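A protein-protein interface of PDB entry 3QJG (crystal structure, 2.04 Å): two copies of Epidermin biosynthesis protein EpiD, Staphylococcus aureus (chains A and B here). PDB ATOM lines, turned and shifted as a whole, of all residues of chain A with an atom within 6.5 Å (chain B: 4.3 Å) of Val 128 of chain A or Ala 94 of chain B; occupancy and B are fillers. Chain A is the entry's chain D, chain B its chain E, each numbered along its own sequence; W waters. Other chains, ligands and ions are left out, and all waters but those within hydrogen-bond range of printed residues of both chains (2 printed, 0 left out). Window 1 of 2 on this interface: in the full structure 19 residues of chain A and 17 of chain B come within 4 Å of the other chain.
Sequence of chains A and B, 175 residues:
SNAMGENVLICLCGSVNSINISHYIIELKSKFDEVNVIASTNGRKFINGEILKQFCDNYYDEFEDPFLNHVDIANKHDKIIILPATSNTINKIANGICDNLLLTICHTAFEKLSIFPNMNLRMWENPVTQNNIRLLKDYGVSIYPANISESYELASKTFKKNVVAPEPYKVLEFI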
ATOM      1  N   ASN A  91      28.342   2.188  -6.929  1.00  0.00           N
ATOM      2  CA  ASN A  91      28.140   3.606  -6.846  1.00  0.00           C
ATOM      3  C   ASN A  91      28.663   4.284  -8.165  1.00  0.00           C
ATOM      4  O   ASN A  91      28.009   5.152  -8.726  1.00  0.00           O
ATOM      5  CB  ASN A  91      28.767   4.172  -5.564  1.00  0.00           C
ATOM      6  CG  ASN A  91      28.079   3.689  -4.319  1.00  0.00           C
ATOM      7  OD1 ASN A  91      26.851   3.743  -4.213  1.00  0.00           O
ATOM      8  ND2 ASN A  91      28.854   3.220  -3.358  1.00  0.00           N
ATOM      9  N   ASN A  95      26.396   6.345 -11.036  1.00  0.00           N
ATOM     10  CA  ASN A  95      26.788   7.707 -11.415  1.00  0.00           C
ATOM     11  C   ASN A  95      27.318   7.819 -12.860  1.00  0.00           C
ATOM     12  O   ASN A  95      27.728   8.885 -13.270  1.00  0.00           O
ATOM     13  CB  ASN A  95      27.800   8.259 -10.416  1.00  0.00           C
ATOM     14  CG  ASN A  95      27.151   8.747  -9.124  1.00  0.00           C
ATOM     15  OD1 ASN A  95      26.387   9.719  -9.135  1.00  0.00           O
ATOM     16  ND2 ASN A  95      27.465   8.076  -7.993  1.00  0.00           N
ATOM     17  N   GLU A 125      24.679   0.055   4.355  1.00  0.00           N
ATOM     18  CA  GLU A 125      23.835   1.076   5.013  1.00  0.00           C
ATOM     19  C   GLU A 125      24.349   2.495   4.902  1.00  0.00           C
ATOM     20  O   GLU A 125      23.780   3.413   5.496  1.00  0.00           O
ATOM     21  CB  GLU A 125      23.622   0.698   6.482  1.00  0.00           C
ATOM     22  CG  GLU A 125      22.755  -0.552   6.604  1.00  0.00           C
ATOM     23  CD  GLU A 125      22.682  -1.104   8.004  1.00  0.00           C
ATOM     24  OE1 GLU A 125      23.504  -0.692   8.863  1.00  0.00           O
ATOM     25  OE2 GLU A 125      21.795  -1.964   8.228  1.00  0.00           O
ATOM     26  N   ASN A 126      25.458   2.693   4.179  1.00  0.00           N
ATOM     27  CA  ASN A 126      25.897   4.060   3.853  1.00  0.00           C
ATOM     28  C   ASN A 126      24.774   4.658   3.002  1.00  0.00           C
ATOM     29  O   ASN A 126      24.295   4.006   2.065  1.00  0.00           O
ATOM     30  CB  ASN A 126      27.254   4.065   3.146  1.00  0.00           C
ATOM     31  CG  ASN A 126      27.704   5.469   2.784  1.00  0.00           C
ATOM     32  OD1 ASN A 126      26.919   6.256   2.213  1.00  0.00           O
ATOM     33  ND2 ASN A 126      28.976   5.793   3.090  1.00  0.00           N
ATOM     34  N   PRO A 127      24.253   5.824   3.400  1.00  0.00           N
ATOM     35  CA  PRO A 127      23.061   6.271   2.697  1.00  0.00           C
ATOM     36  C   PRO A 127      23.233   6.532   1.207  1.00  0.00           C
ATOM     37  O   PRO A 127      22.271   6.390   0.463  1.00  0.00           O
ATOM     38  CB  PRO A 127      22.669   7.585   3.421  1.00  0.00           C
ATOM     39  CG  PRO A 127      23.937   8.018   4.116  1.00  0.00           C
ATOM     40  CD  PRO A 127      24.620   6.725   4.499  1.00  0.00           C
ATOM     41  N   VAL A 128      24.436   6.927   0.797  1.00  0.00           N
ATOM     42  CA  VAL A 128      24.751   7.160  -0.600  1.00  0.00           C
ATOM     43  C   VAL A 128      24.608   5.847  -1.395  1.00  0.00           C
ATOM     44  O   VAL A 128      24.000   5.832  -2.459  1.00  0.00           O
ATOM     45  CB  VAL A 128      26.196   7.702  -0.747  1.00  0.00           C
ATOM     46  CG1 VAL A 128      26.630   7.700  -2.187  1.00  0.00           C
ATOM     47  CG2 VAL A 128      26.306   9.076  -0.136  1.00  0.00           C
ATOM     48  N   THR A 129      25.200   4.765  -0.905  1.00  0.00           N
ATOM     49  CA  THR A 129      24.996   3.429  -1.541  1.00  0.00           C
ATOM     50  C   THR A 129      23.494   3.093  -1.628  1.00  0.00           C
ATOM     51  O   THR A 129      23.065   2.617  -2.661  1.00  0.00           O
ATOM     52  CB  THR A 129      25.741   2.309  -0.833  1.00  0.00           C
ATOM     53  OG1 THR A 129      27.102   2.708  -0.662  1.00  0.00           O
ATOM     54  CG2 THR A 129      25.741   0.969  -1.706  1.00  0.00           C
ATOM     55  N   GLN A 130      22.695   3.451  -0.609  1.00  0.00           N
ATOM     56  CA  GLN A 130      21.263   3.096  -0.619  1.00  0.00           C
ATOM     57  C   GLN A 130      20.527   3.937  -1.657  1.00  0.00           C
ATOM     58  O   GLN A 130      19.706   3.401  -2.387  1.00  0.00           O
ATOM     59  CB  GLN A 130      20.590   3.263   0.743  1.00  0.00           C
ATOM     60  CG  GLN A 130      21.079   2.361   1.895  1.00  0.00           C
ATOM     61  CD  GLN A 130      20.532   2.812   3.280  1.00  0.00           C
ATOM     62  OE1 GLN A 130      20.268   1.977   4.162  1.00  0.00           O
ATOM     63  NE2 GLN A 130      20.349   4.137   3.462  1.00  0.00           N
ATOM     64  N   ASN A 131      20.822   5.247  -1.705  1.00  0.00           N
ATOM     65  CA  ASN A 131      20.348   6.144  -2.768  1.00  0.00           C
ATOM     66  C   ASN A 131      20.650   5.646  -4.151  1.00  0.00           C
ATOM     67  O   ASN A 131      19.773   5.575  -5.002  1.00  0.00           O
ATOM     68  CB  ASN A 131      20.975   7.509  -2.611  1.00  0.00           C
ATOM     69  CG  ASN A 131      20.350   8.307  -1.467  1.00  0.00           C
ATOM     70  OD1 ASN A 131      19.637   7.757  -0.640  1.00  0.00           O
ATOM     71  ND2 ASN A 131      20.628   9.595  -1.418  1.00  0.00           N
ATOM     72  N   ASN A 132      21.897   5.270  -4.368  1.00  0.00           N
ATOM     73  CA  ASN A 132      22.317   4.732  -5.659  1.00  0.00           C
ATOM     74  C   ASN A 132      21.689   3.419  -6.045  1.00  0.00           C
ATOM     75  O   ASN A 132      21.462   3.181  -7.238  1.00  0.00           O
ATOM     76  CB  ASN A 132      23.832   4.574  -5.684  1.00  0.00           C
ATOM     77  CG  ASN A 132      24.548   5.896  -5.813  1.00  0.00           C
ATOM     78  OD1 ASN A 132      23.959   6.909  -6.184  1.00  0.00           O
ATOM     79  ND2 ASN A 132      25.818   5.896  -5.520  1.00  0.00           N
ATOM     80  N   ILE A 133      21.465   2.534  -5.062  1.00  0.00           N
ATOM     81  CA  ILE A 133      20.710   1.285  -5.274  1.00  0.00           C
ATOM     82  C   ILE A 133      19.305   1.646  -5.729  1.00  0.00           C
ATOM     83  O   ILE A 133      18.772   1.073  -6.663  1.00  0.00           O
ATOM     84  CB  ILE A 133      20.631   0.404  -3.967  1.00  0.00           C
ATOM     85  CG1 ILE A 133      21.970  -0.318  -3.657  1.00  0.00           C
ATOM     86  CG2 ILE A 133      19.512  -0.616  -4.055  1.00  0.00           C
ATOM     87  CD1 ILE A 133      22.449  -1.271  -4.766  1.00  0.00           C
ATOM     88  N   ILE B  90      36.670  14.864  -2.029  1.00  0.00           N
ATOM     89  CA  ILE B  90      35.430  15.278  -1.415  1.00  0.00           C
ATOM     90  C   ILE B  90      34.274  14.763  -2.301  1.00  0.00           C
ATOM     91  O   ILE B  90      33.364  14.068  -1.823  1.00  0.00           O
ATOM     92  CB  ILE B  90      35.431  16.782  -1.272  1.00  0.00           C
ATOM     93  CG1 ILE B  90      36.390  17.136  -0.128  1.00  0.00           C
ATOM     94  CG2 ILE B  90      33.984  17.311  -1.007  1.00  0.00           C
ATOM     95  CD1 ILE B  90      36.417  18.657   0.288  1.00  0.00           C
ATOM     96  N   ASN B  91      34.389  15.026  -3.611  1.00  0.00           N
ATOM     97  CA  ASN B  91      33.352  14.698  -4.567  1.00  0.00           C
ATOM     98  C   ASN B  91      33.176  13.207  -4.782  1.00  0.00           C
ATOM     99  O   ASN B  91      32.107  12.738  -5.158  1.00  0.00           O
ATOM    100  CB  ASN B  91      33.643  15.408  -5.892  1.00  0.00           C
ATOM    101  CG  ASN B  91      33.459  16.911  -5.776  1.00  0.00           C
ATOM    102  OD1 ASN B  91      32.752  17.365  -4.896  1.00  0.00           O
ATOM    103  ND2 ASN B  91      34.106  17.687  -6.652  1.00  0.00           N
ATOM    104  N   LYS B  92      34.224  12.447  -4.549  1.00  0.00           N
ATOM    105  CA  LYS B  92      34.115  11.001  -4.674  1.00  0.00           C
ATOM    106  C   LYS B  92      33.457  10.466  -3.400  1.00  0.00           C
ATOM    107  O   LYS B  92      32.624   9.571  -3.469  1.00  0.00           O
ATOM    108  CB  LYS B  92      35.472  10.347  -4.919  1.00  0.00           C
ATOM    109  CG  LYS B  92      35.978  10.351  -6.405  1.00  0.00           C
ATOM    110  CD  LYS B  92      37.044   9.272  -6.589  1.00  0.00           C
ATOM    111  CE  LYS B  92      37.954   9.404  -7.779  1.00  0.00           C
ATOM    112  NZ  LYS B  92      39.022   8.278  -7.895  1.00  0.00           N
ATOM    113  N   ILE B  93      33.810  10.994  -2.236  1.00  0.00           N
ATOM    114  CA  ILE B  93      33.214  10.483  -1.000  1.00  0.00           C
ATOM    115  C   ILE B  93      31.714  10.675  -1.135  1.00  0.00           C
ATOM    116  O   ILE B  93      30.944   9.717  -0.925  1.00  0.00           O
ATOM    117  CB  ILE B  93      33.733  11.176   0.266  1.00  0.00           C
ATOM    118  CG1 ILE B  93      35.273  11.127   0.337  1.00  0.00           C
ATOM    119  CG2 ILE B  93      33.184  10.526   1.455  1.00  0.00           C
ATOM    120  CD1 ILE B  93      35.836  10.171   1.257  1.00  0.00           C
ATOM    121  N   ALA B  94      31.304  11.849  -1.615  1.00  0.00           N
ATOM    122  CA  ALA B  94      29.869  12.244  -1.585  1.00  0.00           C
ATOM    123  C   ALA B  94      29.057  11.389  -2.538  1.00  0.00           C
ATOM    124  O   ALA B  94      27.832  11.345  -2.437  1.00  0.00           O
ATOM    125  CB  ALA B  94      29.702  13.690  -1.927  1.00  0.00           C
ATOM    126  N   ASN B  95      29.736  10.743  -3.488  1.00  0.00           N
ATOM    127  CA  ASN B  95      29.085   9.884  -4.476  1.00  0.00           C
ATOM    128  C   ASN B  95      29.330   8.392  -4.272  1.00  0.00           C
ATOM    129  O   ASN B  95      28.945   7.587  -5.125  1.00  0.00           O
ATOM    130  CB  ASN B  95      29.545  10.252  -5.884  1.00  0.00           C
ATOM    131  CG  ASN B  95      28.884  11.526  -6.386  1.00  0.00           C
ATOM    132  OD1 ASN B  95      27.691  11.524  -6.693  1.00  0.00           O
ATOM    133  ND2 ASN B  95      29.649  12.614  -6.472  1.00  0.00           N
ATOM    134  N   GLY B  96      29.942   8.040  -3.137  1.00  0.00           N
ATOM    135  CA  GLY B  96      30.179   6.674  -2.721  1.00  0.00           C
ATOM    136  C   GLY B  96      31.211   5.914  -3.513  1.00  0.00           C
ATOM    137  O   GLY B  96      31.292   4.681  -3.453  1.00  0.00           O
ATOM    138  N   ASN B 132      27.945  18.666  -3.013  1.00  0.00           N
ATOM    139  CA  ASN B 132      28.483  17.478  -2.381  1.00  0.00           C
ATOM    140  C   ASN B 132      28.849  17.748  -0.920  1.00  0.00           C
ATOM    141  O   ASN B 132      28.634  16.895  -0.056  1.00  0.00           O
ATOM    142  CB  ASN B 132      29.659  16.928  -3.199  1.00  0.00           C
ATOM    143  CG  ASN B 132      29.197  16.242  -4.506  1.00  0.00           C
ATOM    144  OD1 ASN B 132      28.038  15.864  -4.637  1.00  0.00           O
ATOM    145  ND2 ASN B 132      30.106  16.066  -5.447  1.00  0.00           N
ATOM    146  N   LEU B 136      27.131  15.674   2.312  1.00  0.00           N
ATOM    147  CA  LEU B 136      27.926  15.038   3.357  1.00  0.00           C
ATOM    148  C   LEU B 136      27.542  15.535   4.747  1.00  0.00           C
ATOM    149  O   LEU B 136      27.420  14.744   5.688  1.00  0.00           O
ATOM    150  CB  LEU B 136      29.405  15.296   3.107  1.00  0.00           C
ATOM    151  CG  LEU B 136      29.983  14.622   1.873  1.00  0.00           C
ATOM    152  CD1 LEU B 136      31.289  15.275   1.550  1.00  0.00           C
ATOM    153  CD2 LEU B 136      30.163  13.109   2.071  1.00  0.00           C
ATOM    154  N   TYR B 139      24.570  13.742   5.603  1.00  0.00           N
ATOM    155  CA  TYR B 139      24.820  12.341   5.944  1.00  0.00           C
ATOM    156  C   TYR B 139      25.770  12.146   7.122  1.00  0.00           C
ATOM    157  O   TYR B 139      26.299  11.043   7.320  1.00  0.00           O
ATOM    158  CB  TYR B 139      25.344  11.563   4.725  1.00  0.00           C
ATOM    159  CG  TYR B 139      24.338  11.436   3.611  1.00  0.00           C
ATOM    160  CD1 TYR B 139      22.997  11.168   3.890  1.00  0.00           C
ATOM    161  CD2 TYR B 139      24.721  11.555   2.280  1.00  0.00           C
ATOM    162  CE1 TYR B 139      22.048  11.044   2.868  1.00  0.00           C
ATOM    163  CE2 TYR B 139      23.786  11.434   1.242  1.00  0.00           C
ATOM    164  CZ  TYR B 139      22.457  11.170   1.544  1.00  0.00           C
ATOM    165  OH  TYR B 139      21.501  11.047   0.552  1.00  0.00           O
HETATM  166  O   HOH W   1      25.865   9.106  -6.190  1.00  0.00           O
HETATM  167  O   HOH W   2      25.622  12.177  -8.086  1.00  0.00           O
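The side-chain amide nitrogen of Asn 91 of chain A sits at hydrogen-bond distance from the backbone carbonyl oxygen of Gly 96 of chain B.
ND2 of Asn 95 of chain A sits at hydrogen-bond distance from O of Asn 95 of chain B, at 3.3 Å.
ND2 of Asn 131 of chain A sits at hydrogen-bond distance from OH of Tyr 139 of chain B.
The backbone carbonyl oxygen of Asn 91 of chain A is in hydrogen-bond range of the side-chain amide nitrogen of Asn 95 of chain A.
ND2 of Asn 91 of chain A sits at hydrogen-bond distance from OG1 of Thr 129 of chain A.
The side-chain amide oxygen of Asn 91 of chain A is in hydrogen-bond range of the side-chain amide nitrogen of Asn 132 of chain A, 2.7 Å away.
The side-chain amide oxygen (OD1) of Asn 126 of chain A lies within hydrogen-bond range of the backbone NH (N) of Val 128 of chain A, 2.9 Å away.
The side-chain amide oxygen of Asn 131 of chain A sits close to the backbone carbonyl oxygen of Pro 127 of chain A (3.2 Å).
O of Asn 91 of chain B sits at hydrogen-bond distance from ND2 of Asn 95 of chain B (2.8 Å).
CB of Asn 91 of chain A touches O of Asn 95 of chain B, 3.4 Å away.
CD1 of Tyr 139 of chain B touches CG of Pro 127 of chain A (3.3 Å).
Val 128 of chain A touches Ala 94 of chain B (CG2 to O, 3.6 Å).
Val 128 of chain A touches Asn 95 of chain B (CG1 to C, 3.5 Å).
Val 128 of chain A touches Gly 96 of chain B.
Tyr 139 of chain B touches Val 128 of chain A (CE2 to CG2, 3.7 Å).
Asn 95 of chain B touches Asn 132 of chain A (O to ND2, 3.6 Å).
Printed residues of chain B within 4 Å of Val 128 of chain A: Ala 94 (3.6 Å), Asn 95 (3.5 Å), Gly 96 (3.5 Å) and Tyr 139 (3.7 Å).
Of the printed residues of chain B, Asn 132 of chain A touches Asn 95.
Printed residues of chain B within 4 Å of Pro 127 of chain A: Tyr 139.
Of the printed residues of chain B, Asn 95 of chain A touches Asn 95 (3.3 Å).
Printed residues of chain A within 4 Å of Tyr 139 of chain B: Pro 127, Val 128 and Asn 131.
The nearest printed residue of chain B that does not touch Asn 91 of chain A is Lys 92 of chain B (7.0 Å).
Hydrophobic or aromatic side chains of chain B that line the printed part of chain A: Tyr 139.
Of the 11 printed residues of chain A, 6 touch a printed residue of chain B.
Asn 91 of chain A touches Asn 95 of chain B, but with the chains exchanged Asn 95 of chain A does not touch Asn 91 of chain B (7.2 Å).
Asn 95 of chain A touches its own counterpart, Asn 95 of chain B.
Asn 132 of chain A touches Asn 95 of chain B, but with the chains exchanged Asn 95 of chain A does not touch Asn 132 of chain B (7.8 Å).
3 positions are printed for both chains.
Water W2 bridges the side-chain amide oxygen (OD1) of Asn 95 of chain B (2.6 Å) and the side-chain amide oxygen (OD1) of Asn 95 of chain A (2.8 Å).
Water W1 lies within hydrogen-bond range of the side-chain amide nitrogen of Asn 95 of chain A (2.6 Å), the side-chain amide oxygen of Asn 132 of chain A (2.9 Å) and the side-chain amide oxygen of Asn 95 of chain B (3.1 Å).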
